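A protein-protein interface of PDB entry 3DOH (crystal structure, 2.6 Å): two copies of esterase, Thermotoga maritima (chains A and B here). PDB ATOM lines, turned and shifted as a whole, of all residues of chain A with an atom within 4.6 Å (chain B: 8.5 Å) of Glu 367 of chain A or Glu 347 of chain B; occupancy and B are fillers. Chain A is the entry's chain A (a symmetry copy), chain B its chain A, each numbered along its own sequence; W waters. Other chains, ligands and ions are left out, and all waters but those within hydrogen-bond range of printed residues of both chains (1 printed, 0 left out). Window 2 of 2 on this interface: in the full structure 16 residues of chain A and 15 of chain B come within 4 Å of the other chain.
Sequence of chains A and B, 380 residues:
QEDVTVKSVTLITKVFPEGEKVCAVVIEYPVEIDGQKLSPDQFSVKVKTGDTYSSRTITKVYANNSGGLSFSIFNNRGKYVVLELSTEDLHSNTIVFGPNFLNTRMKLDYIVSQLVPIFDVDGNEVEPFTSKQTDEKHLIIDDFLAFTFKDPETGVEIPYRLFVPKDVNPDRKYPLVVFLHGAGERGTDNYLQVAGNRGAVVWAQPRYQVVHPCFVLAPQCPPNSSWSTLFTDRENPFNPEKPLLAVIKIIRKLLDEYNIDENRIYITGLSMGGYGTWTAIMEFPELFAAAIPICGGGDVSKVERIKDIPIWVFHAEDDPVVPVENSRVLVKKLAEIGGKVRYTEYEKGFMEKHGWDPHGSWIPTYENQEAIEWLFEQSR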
ATOM      1  N   PRO A  17      -1.541   5.068  26.698  1.00  0.00           N
ATOM      2  CA  PRO A  17      -1.652   5.722  27.998  1.00  0.00           C
ATOM      3  C   PRO A  17      -2.742   5.146  28.921  1.00  0.00           C
ATOM      4  O   PRO A  17      -2.550   5.111  30.143  1.00  0.00           O
ATOM      5  CB  PRO A  17      -1.886   7.189  27.620  1.00  0.00           C
ATOM      6  CG  PRO A  17      -1.126   7.333  26.310  1.00  0.00           C
ATOM      7  CD  PRO A  17      -1.495   6.054  25.589  1.00  0.00           C
ATOM      8  N   ARG A 198       1.380   3.360  31.106  1.00  0.00           N
ATOM      9  CA  ARG A 198       2.685   3.485  30.470  1.00  0.00           C
ATOM     10  C   ARG A 198       3.769   3.636  31.545  1.00  0.00           C
ATOM     11  O   ARG A 198       4.915   4.008  31.270  1.00  0.00           O
ATOM     12  CB  ARG A 198       2.700   4.660  29.468  1.00  0.00           C
ATOM     13  CG  ARG A 198       2.142   4.390  28.022  1.00  0.00           C
ATOM     14  CD  ARG A 198       3.015   5.060  26.905  1.00  0.00           C
ATOM     15  NE  ARG A 198       3.005   4.293  25.637  1.00  0.00           N
ATOM     16  CZ  ARG A 198       2.413   4.672  24.473  1.00  0.00           C
ATOM     17  NH1 ARG A 198       1.763   5.851  24.361  1.00  0.00           N
ATOM     18  NH2 ARG A 198       2.461   3.870  23.385  1.00  0.00           N
ATOM     19  N   ARG A 207      12.806   5.804  21.930  1.00  0.00           N
ATOM     20  CA  ARG A 207      13.047   7.284  21.970  1.00  0.00           C
ATOM     21  C   ARG A 207      13.817   7.753  23.214  1.00  0.00           C
ATOM     22  O   ARG A 207      14.607   8.707  23.145  1.00  0.00           O
ATOM     23  CB  ARG A 207      11.745   8.096  21.805  1.00  0.00           C
ATOM     24  CG  ARG A 207      10.683   7.847  22.899  1.00  0.00           C
ATOM     25  CD  ARG A 207       9.403   8.646  22.669  1.00  0.00           C
ATOM     26  NE  ARG A 207       9.053   8.536  21.268  1.00  0.00           N
ATOM     27  CZ  ARG A 207       8.249   7.589  20.791  1.00  0.00           C
ATOM     28  NH1 ARG A 207       7.703   6.713  21.644  1.00  0.00           N
ATOM     29  NH2 ARG A 207       7.977   7.527  19.477  1.00  0.00           N
ATOM     30  N   ILE A 363      -1.664   9.329  33.382  1.00  0.00           N
ATOM     31  CA  ILE A 363      -1.744   9.401  31.920  1.00  0.00           C
ATOM     32  C   ILE A 363      -1.076  10.642  31.287  1.00  0.00           C
ATOM     33  O   ILE A 363      -0.181  10.497  30.477  1.00  0.00           O
ATOM     34  CB  ILE A 363      -3.197   9.280  31.464  1.00  0.00           C
ATOM     35  CG1 ILE A 363      -3.714   7.865  31.788  1.00  0.00           C
ATOM     36  CG2 ILE A 363      -3.315   9.643  29.990  1.00  0.00           C
ATOM     37  CD1 ILE A 363      -5.232   7.755  31.958  1.00  0.00           C
ATOM     38  N   PRO A 364      -1.477  11.863  31.651  1.00  0.00           N
ATOM     39  CA  PRO A 364      -0.666  12.923  31.052  1.00  0.00           C
ATOM     40  C   PRO A 364       0.747  12.950  31.581  1.00  0.00           C
ATOM     41  O   PRO A 364       1.657  13.455  30.903  1.00  0.00           O
ATOM     42  CB  PRO A 364      -1.361  14.211  31.492  1.00  0.00           C
ATOM     43  CG  PRO A 364      -2.362  13.821  32.470  1.00  0.00           C
ATOM     44  CD  PRO A 364      -2.569  12.374  32.481  1.00  0.00           C
ATOM     45  N   THR A 365       0.942  12.454  32.797  1.00  0.00           N
ATOM     46  CA  THR A 365       2.228  12.611  33.453  1.00  0.00           C
ATOM     47  C   THR A 365       3.291  11.817  32.724  1.00  0.00           C
ATOM     48  O   THR A 365       4.327  12.367  32.395  1.00  0.00           O
ATOM     49  CB  THR A 365       2.124  12.190  34.902  1.00  0.00           C
ATOM     50  OG1 THR A 365       1.141  13.021  35.513  1.00  0.00           O
ATOM     51  CG2 THR A 365       3.418  12.352  35.609  1.00  0.00           C
ATOM     52  N   TYR A 366       3.023  10.538  32.451  1.00  0.00           N
ATOM     53  CA  TYR A 366       3.967   9.713  31.698  1.00  0.00           C
ATOM     54  C   TYR A 366       4.098  10.141  30.247  1.00  0.00           C
ATOM     55  O   TYR A 366       5.025   9.710  29.542  1.00  0.00           O
ATOM     56  CB  TYR A 366       3.672   8.207  31.842  1.00  0.00           C
ATOM     57  CG  TYR A 366       3.933   7.742  33.258  1.00  0.00           C
ATOM     58  CD1 TYR A 366       5.113   8.101  33.909  1.00  0.00           C
ATOM     59  CD2 TYR A 366       2.992   6.973  33.971  1.00  0.00           C
ATOM     60  CE1 TYR A 366       5.361   7.694  35.225  1.00  0.00           C
ATOM     61  CE2 TYR A 366       3.249   6.583  35.306  1.00  0.00           C
ATOM     62  CZ  TYR A 366       4.438   6.941  35.901  1.00  0.00           C
ATOM     63  OH  TYR A 366       4.720   6.583  37.185  1.00  0.00           O
ATOM     64  N   GLU A 367       3.199  11.012  29.808  1.00  0.00           N
ATOM     65  CA  GLU A 367       3.311  11.606  28.470  1.00  0.00           C
ATOM     66  C   GLU A 367       4.076  12.944  28.472  1.00  0.00           C
ATOM     67  O   GLU A 367       4.251  13.568  27.427  1.00  0.00           O
ATOM     68  CB  GLU A 367       1.941  11.682  27.757  1.00  0.00           C
ATOM     69  CG  GLU A 367       1.295  10.319  27.406  1.00  0.00           C
ATOM     70  CD  GLU A 367       2.212   9.351  26.594  1.00  0.00           C
ATOM     71  OE1 GLU A 367       2.446   9.601  25.389  1.00  0.00           O
ATOM     72  OE2 GLU A 367       2.681   8.318  27.159  1.00  0.00           O
ATOM     73  N   ASN A 368       4.617  13.333  29.614  1.00  0.00           N
ATOM     74  CA  ASN A 368       5.334  14.596  29.727  1.00  0.00           C
ATOM     75  C   ASN A 368       6.863  14.455  29.524  1.00  0.00           C
ATOM     76  O   ASN A 368       7.591  13.972  30.422  1.00  0.00           O
ATOM     77  CB  ASN A 368       5.010  15.164  31.098  1.00  0.00           C
ATOM     78  CG  ASN A 368       5.515  16.576  31.309  1.00  0.00           C
ATOM     79  OD1 ASN A 368       6.567  16.983  30.783  1.00  0.00           O
ATOM     80  ND2 ASN A 368       4.784  17.324  32.153  1.00  0.00           N
ATOM     81  N   GLN A 369       7.350  14.877  28.353  1.00  0.00           N
ATOM     82  CA  GLN A 369       8.776  14.739  27.993  1.00  0.00           C
ATOM     83  C   GLN A 369       9.663  15.510  28.981  1.00  0.00           C
ATOM     84  O   GLN A 369      10.782  15.092  29.265  1.00  0.00           O
ATOM     85  CB  GLN A 369       9.066  15.103  26.495  1.00  0.00           C
ATOM     86  CG  GLN A 369      10.593  15.286  26.186  1.00  0.00           C
ATOM     87  CD  GLN A 369      10.999  15.289  24.681  1.00  0.00           C
ATOM     88  OE1 GLN A 369      10.250  15.756  23.816  1.00  0.00           O
ATOM     89  NE2 GLN A 369      12.217  14.784  24.382  1.00  0.00           N
ATOM     90  N   HIS B 315      12.670  13.307  14.494  1.00  0.00           N
ATOM     91  CA  HIS B 315      12.265  12.275  13.538  1.00  0.00           C
ATOM     92  C   HIS B 315      10.915  11.753  14.034  1.00  0.00           C
ATOM     93  O   HIS B 315      10.614  11.840  15.214  1.00  0.00           O
ATOM     94  CB  HIS B 315      13.283  11.130  13.567  1.00  0.00           C
ATOM     95  CG  HIS B 315      13.473  10.439  12.251  1.00  0.00           C
ATOM     96  ND1 HIS B 315      12.429   9.889  11.534  1.00  0.00           N
ATOM     97  CD2 HIS B 315      14.596  10.165  11.548  1.00  0.00           C
ATOM     98  CE1 HIS B 315      12.901   9.336  10.434  1.00  0.00           C
ATOM     99  NE2 HIS B 315      14.214   9.475  10.430  1.00  0.00           N
ATOM    100  N   ALA B 316      10.085  11.208  13.158  1.00  0.00           N
ATOM    101  CA  ALA B 316       8.849  10.590  13.633  1.00  0.00           C
ATOM    102  C   ALA B 316       9.047   9.107  13.541  1.00  0.00           C
ATOM    103  O   ALA B 316       9.566   8.603  12.524  1.00  0.00           O
ATOM    104  CB  ALA B 316       7.668  11.008  12.808  1.00  0.00           C
ATOM    105  N   GLU B 317       8.606   8.416  14.602  1.00  0.00           N
ATOM    106  CA  GLU B 317       8.705   6.959  14.724  1.00  0.00           C
ATOM    107  C   GLU B 317       8.231   6.189  13.488  1.00  0.00           C
ATOM    108  O   GLU B 317       8.868   5.215  13.065  1.00  0.00           O
ATOM    109  CB  GLU B 317       7.903   6.508  15.923  1.00  0.00           C
ATOM    110  CG  GLU B 317       8.114   5.043  16.242  1.00  0.00           C
ATOM    111  CD  GLU B 317       7.213   4.134  15.424  1.00  0.00           C
ATOM    112  OE1 GLU B 317       6.246   4.624  14.803  1.00  0.00           O
ATOM    113  OE2 GLU B 317       7.474   2.928  15.382  1.00  0.00           O
ATOM    114  N   ASP B 318       7.100   6.626  12.940  1.00  0.00           N
ATOM    115  CA  ASP B 318       6.492   5.987  11.781  1.00  0.00           C
ATOM    116  C   ASP B 318       6.766   6.699  10.472  1.00  0.00           C
ATOM    117  O   ASP B 318       5.918   6.627   9.590  1.00  0.00           O
ATOM    118  CB  ASP B 318       4.967   5.880  11.955  1.00  0.00           C
ATOM    119  CG  ASP B 318       4.341   7.165  12.427  1.00  0.00           C
ATOM    120  OD1 ASP B 318       5.057   8.162  12.681  1.00  0.00           O
ATOM    121  OD2 ASP B 318       3.123   7.185  12.577  1.00  0.00           O
ATOM    122  N   ASP B 319       7.902   7.405  10.338  1.00  0.00           N
ATOM    123  CA  ASP B 319       8.278   7.982   9.030  1.00  0.00           C
ATOM    124  C   ASP B 319       8.441   6.826   8.018  1.00  0.00           C
ATOM    125  O   ASP B 319       9.310   5.988   8.202  1.00  0.00           O
ATOM    126  CB  ASP B 319       9.558   8.835   9.135  1.00  0.00           C
ATOM    127  CG  ASP B 319       9.995   9.464   7.786  1.00  0.00           C
ATOM    128  OD1 ASP B 319       9.607   8.999   6.688  1.00  0.00           O
ATOM    129  OD2 ASP B 319      10.782  10.429   7.824  1.00  0.00           O
ATOM    130  N   VAL B 324      13.140   5.745  11.096  1.00  0.00           N
ATOM    131  CA  VAL B 324      13.493   6.573  12.266  1.00  0.00           C
ATOM    132  C   VAL B 324      14.840   6.086  12.830  1.00  0.00           C
ATOM    133  O   VAL B 324      15.581   6.841  13.504  1.00  0.00           O
ATOM    134  CB  VAL B 324      12.361   6.538  13.339  1.00  0.00           C
ATOM    135  CG1 VAL B 324      12.101   5.093  13.829  1.00  0.00           C
ATOM    136  CG2 VAL B 324      12.646   7.457  14.519  1.00  0.00           C
ATOM    137  N   ARG B 328      17.923   7.518  15.392  1.00  0.00           N
ATOM    138  CA  ARG B 328      18.266   6.740  16.598  1.00  0.00           C
ATOM    139  C   ARG B 328      19.704   6.295  16.654  1.00  0.00           C
ATOM    140  O   ARG B 328      20.330   6.380  17.727  1.00  0.00           O
ATOM    141  CB  ARG B 328      17.380   5.514  16.794  1.00  0.00           C
ATOM    142  CG  ARG B 328      16.002   5.848  17.176  1.00  0.00           C
ATOM    143  CD  ARG B 328      15.195   4.682  16.990  1.00  0.00           C
ATOM    144  NE  ARG B 328      13.796   4.933  17.243  1.00  0.00           N
ATOM    145  CZ  ARG B 328      12.876   3.980  17.301  1.00  0.00           C
ATOM    146  NH1 ARG B 328      13.231   2.708  17.162  1.00  0.00           N
ATOM    147  NH2 ARG B 328      11.603   4.302  17.493  1.00  0.00           N
ATOM    148  N   THR B 344      13.956  14.434  20.300  1.00  0.00           N
ATOM    149  CA  THR B 344      12.531  14.339  20.365  1.00  0.00           C
ATOM    150  C   THR B 344      12.142  13.423  19.206  1.00  0.00           C
ATOM    151  O   THR B 344      12.416  13.758  18.055  1.00  0.00           O
ATOM    152  CB  THR B 344      11.952  15.729  20.110  1.00  0.00           C
ATOM    153  OG1 THR B 344      12.501  16.632  21.066  1.00  0.00           O
ATOM    154  CG2 THR B 344      10.440  15.729  20.228  1.00  0.00           C
ATOM    155  N   GLU B 345      11.528  12.274  19.501  1.00  0.00           N
ATOM    156  CA  GLU B 345      11.008  11.376  18.472  1.00  0.00           C
ATOM    157  C   GLU B 345       9.511  11.287  18.591  1.00  0.00           C
ATOM    158  O   GLU B 345       8.990  10.654  19.526  1.00  0.00           O
ATOM    159  CB  GLU B 345      11.586   9.990  18.604  1.00  0.00           C
ATOM    160  CG  GLU B 345      11.132   9.014  17.530  1.00  0.00           C
ATOM    161  CD  GLU B 345      11.605   7.577  17.797  1.00  0.00           C
ATOM    162  OE1 GLU B 345      12.826   7.344  17.956  1.00  0.00           O
ATOM    163  OE2 GLU B 345      10.749   6.666  17.868  1.00  0.00           O
ATOM    164  N   TYR B 346       8.832  11.918  17.642  1.00  0.00           N
ATOM    165  CA  TYR B 346       7.384  11.892  17.541  1.00  0.00           C
ATOM    166  C   TYR B 346       6.791  10.468  17.469  1.00  0.00           C
ATOM    167  O   TYR B 346       7.061   9.723  16.518  1.00  0.00           O
ATOM    168  CB  TYR B 346       6.923  12.733  16.325  1.00  0.00           C
ATOM    169  CG  TYR B 346       7.379  14.177  16.369  1.00  0.00           C
ATOM    170  CD1 TYR B 346       6.828  15.062  17.297  1.00  0.00           C
ATOM    171  CD2 TYR B 346       8.357  14.657  15.490  1.00  0.00           C
ATOM    172  CE1 TYR B 346       7.234  16.394  17.377  1.00  0.00           C
ATOM    173  CE2 TYR B 346       8.778  15.999  15.541  1.00  0.00           C
ATOM    174  CZ  TYR B 346       8.200  16.860  16.499  1.00  0.00           C
ATOM    175  OH  TYR B 346       8.580  18.172  16.602  1.00  0.00           O
ATOM    176  N   GLU B 347       5.994  10.120  18.489  1.00  0.00           N
ATOM    177  CA  GLU B 347       5.277   8.838  18.572  1.00  0.00           C
ATOM    178  C   GLU B 347       4.439   8.504  17.327  1.00  0.00           C
ATOM    179  O   GLU B 347       3.801   9.392  16.736  1.00  0.00           O
ATOM    180  CB  GLU B 347       4.288   8.855  19.731  1.00  0.00           C
ATOM    181  CG  GLU B 347       4.842   8.741  21.105  1.00  0.00           C
ATOM    182  CD  GLU B 347       3.689   8.750  22.148  1.00  0.00           C
ATOM    183  OE1 GLU B 347       3.147   9.862  22.408  1.00  0.00           O
ATOM    184  OE2 GLU B 347       3.318   7.647  22.685  1.00  0.00           O
ATOM    185  N   LYS B 348       4.407   7.210  17.000  1.00  0.00           N
ATOM    186  CA  LYS B 348       3.488   6.646  16.002  1.00  0.00           C
ATOM    187  C   LYS B 348       2.108   7.222  16.164  1.00  0.00           C
ATOM    188  O   LYS B 348       1.588   7.257  17.275  1.00  0.00           O
ATOM    189  CB  LYS B 348       3.388   5.137  16.171  1.00  0.00           C
ATOM    190  CG  LYS B 348       2.394   4.474  15.214  1.00  0.00           C
ATOM    191  CD  LYS B 348       2.621   2.982  15.082  1.00  0.00           C
ATOM    192  CE  LYS B 348       1.630   2.409  14.100  1.00  0.00           C
ATOM    193  NZ  LYS B 348       2.083   2.664  12.719  1.00  0.00           N
ATOM    194  N   GLY B 349       1.518   7.683  15.069  1.00  0.00           N
ATOM    195  CA  GLY B 349       0.210   8.311  15.145  1.00  0.00           C
ATOM    196  C   GLY B 349       0.162   9.808  15.472  1.00  0.00           C
ATOM    197  O   GLY B 349      -0.812  10.489  15.106  1.00  0.00           O
ATOM    198  N   PHE B 350       1.180  10.334  16.153  1.00  0.00           N
ATOM    199  CA  PHE B 350       1.188  11.751  16.515  1.00  0.00           C
ATOM    200  C   PHE B 350       0.978  12.686  15.300  1.00  0.00           C
ATOM    201  O   PHE B 350       0.219  13.689  15.359  1.00  0.00           O
ATOM    202  CB  PHE B 350       2.479  12.130  17.234  1.00  0.00           C
ATOM    203  CG  PHE B 350       2.667  13.604  17.393  1.00  0.00           C
ATOM    204  CD1 PHE B 350       2.386  14.223  18.594  1.00  0.00           C
ATOM    205  CD2 PHE B 350       3.116  14.377  16.345  1.00  0.00           C
ATOM    206  CE1 PHE B 350       2.568  15.611  18.758  1.00  0.00           C
ATOM    207  CE2 PHE B 350       3.281  15.753  16.483  1.00  0.00           C
ATOM    208  CZ  PHE B 350       3.017  16.373  17.686  1.00  0.00           C
ATOM    209  N   MET B 351       1.678  12.360  14.215  1.00  0.00           N
ATOM    210  CA  MET B 351       1.620  13.166  13.022  1.00  0.00           C
ATOM    211  C   MET B 351       0.219  13.117  12.406  1.00  0.00           C
ATOM    212  O   MET B 351      -0.403  14.191  12.222  1.00  0.00           O
ATOM    213  CB  MET B 351       2.696  12.732  12.030  1.00  0.00           C
ATOM    214  CG  MET B 351       4.122  12.904  12.549  1.00  0.00           C
ATOM    215  SD  MET B 351       4.631  14.632  12.687  1.00  0.00           S
ATOM    216  CE  MET B 351       4.878  15.014  10.981  1.00  0.00           C
ATOM    217  N   GLU B 352      -0.301  11.903  12.123  1.00  0.00           N
ATOM    218  CA  GLU B 352      -1.615  11.812  11.435  1.00  0.00           C
ATOM    219  C   GLU B 352      -2.711  12.389  12.317  1.00  0.00           C
ATOM    220  O   GLU B 352      -3.642  13.003  11.809  1.00  0.00           O
ATOM    221  CB  GLU B 352      -1.971  10.402  10.937  1.00  0.00           C
ATOM    222  CG  GLU B 352      -0.911   9.742   9.989  1.00  0.00           C
ATOM    223  CD  GLU B 352      -1.063  10.055   8.472  1.00  0.00           C
ATOM    224  OE1 GLU B 352      -1.316  11.241   8.076  1.00  0.00           O
ATOM    225  OE2 GLU B 352      -0.896   9.080   7.671  1.00  0.00           O
ATOM    226  N   LYS B 353      -2.571  12.238  13.632  1.00  0.00           N
ATOM    227  CA  LYS B 353      -3.480  12.886  14.553  1.00  0.00           C
ATOM    228  C   LYS B 353      -3.537  14.379  14.252  1.00  0.00           C
ATOM    229  O   LYS B 353      -4.615  14.938  14.212  1.00  0.00           O
ATOM    230  CB  LYS B 353      -3.095  12.575  16.014  1.00  0.00           C
ATOM    231  CG  LYS B 353      -3.610  13.558  17.092  1.00  0.00           C
ATOM    232  CD  LYS B 353      -3.006  13.284  18.517  1.00  0.00           C
ATOM    233  CE  LYS B 353      -3.922  13.837  19.672  1.00  0.00           C
ATOM    234  NZ  LYS B 353      -3.986  15.349  19.775  1.00  0.00           N
ATOM    235  N   HIS B 354      -2.397  15.022  13.978  1.00  0.00           N
ATOM    236  CA  HIS B 354      -2.377  16.491  13.706  1.00  0.00           C
ATOM    237  C   HIS B 354      -2.573  16.846  12.234  1.00  0.00           C
ATOM    238  O   HIS B 354      -2.458  18.022  11.854  1.00  0.00           O
ATOM    239  CB  HIS B 354      -1.086  17.130  14.189  1.00  0.00           C
ATOM    240  CG  HIS B 354      -0.939  17.162  15.669  1.00  0.00           C
ATOM    241  ND1 HIS B 354      -1.101  18.313  16.403  1.00  0.00           N
ATOM    242  CD2 HIS B 354      -0.632  16.191  16.558  1.00  0.00           C
ATOM    243  CE1 HIS B 354      -0.898  18.054  17.683  1.00  0.00           C
ATOM    244  NE2 HIS B 354      -0.616  16.773  17.804  1.00  0.00           N
ATOM    245  N   PRO B 358       3.407  11.408   8.144  1.00  0.00           N
ATOM    246  CA  PRO B 358       4.469  11.277   9.174  1.00  0.00           C
ATOM    247  C   PRO B 358       5.894  11.586   8.685  1.00  0.00           C
ATOM    248  O   PRO B 358       6.776  11.713   9.486  1.00  0.00           O
ATOM    249  CB  PRO B 358       4.329   9.820   9.714  1.00  0.00           C
ATOM    250  CG  PRO B 358       3.436   9.131   8.835  1.00  0.00           C
ATOM    251  CD  PRO B 358       2.753  10.113   7.871  1.00  0.00           C
HETATM  252  O   HOH W   1      10.855  18.014  22.148  1.00  0.00           O
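OE2 of Glu 345 of chain B is in salt-bridge range of NH2 of Arg 207 of chain A. The guanidinium group (NH1) of Arg 198 of chain A lies within salt-bridge range of the side-chain carboxylate (OE2) of Glu 347 of chain B (2.9 Å). N of Glu 347 of chain B sits close to NH2 of Arg 207 of chain A (3.4 Å). The side-chain carboxylate (OE1) of Glu 367 of chain A sits close to the side-chain carboxylate (OE1) of Glu 347 of chain B, at 3.1 Å.
O of His 315 of chain B lies within hydrogen-bond range of N of Tyr 346 of chain B. N of Glu 317 of chain B lies within hydrogen-bond range of O of Tyr 346 of chain B (2.8 Å). OE2 of Glu 345 of chain B is in salt-bridge range of NH2 of Arg 328 of chain B (2.5 Å). The guanidinium group (NH1) of Arg 198 of chain A lies within salt-bridge range of the side-chain carboxylate (OE2) of Glu 367 of chain A (3.8 Å).
Among the printed residues, merely in contact across the chains: Arg 207 of chain A with Glu 317 of chain B, Arg 207 of chain A with Tyr 346 of chain B and Gln 369 of chain A with Thr 344 of chain B.
Of the printed residues of chain B, Arg 198 of chain A touches Glu 347. Printed residues of chain B within 4 Å of Arg 207 of chain A: Glu 317 (3.7 Å), Glu 345 (2.7 Å), Tyr 346 (3.8 Å) and Glu 347 (3.1 Å). Of the printed residues of chain B, Glu 367 of chain A touches Glu 347. Printed residues of chain A within 4 Å of Glu 317 of chain B: Arg 207. Of the printed residues of chain A, Glu 345 of chain B touches Arg 207. Of the printed residues of chain A, Tyr 346 of chain B touches Arg 207. Of the printed residues of chain A, Glu 347 of chain B touches Arg 198, Arg 207 and Glu 367. Glu 352 of chain B touches none of the printed residues of chain A. The nearest residue of chain B that does not touch Glu 367 of chain A is Phe 350 of chain B (8.2 Å). The nearest printed residue of chain A that does not touch Tyr 346 of chain B is Gln 369 of chain A (7.1 Å).
Printed residues of chain A that touch a printed residue of chain B: Arg 198, Arg 207, Glu 367 and Gln 369.
No position is printed for both chains. Of the 7 pairs that touch across the chains among the printed residues, none has its exchanged pair printed and touching as well.
Water W1 lies within hydrogen-bond range of the side-chain hydroxyl of Thr 344 of chain B and the side-chain amide oxygen of Gln 369 of chain A.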
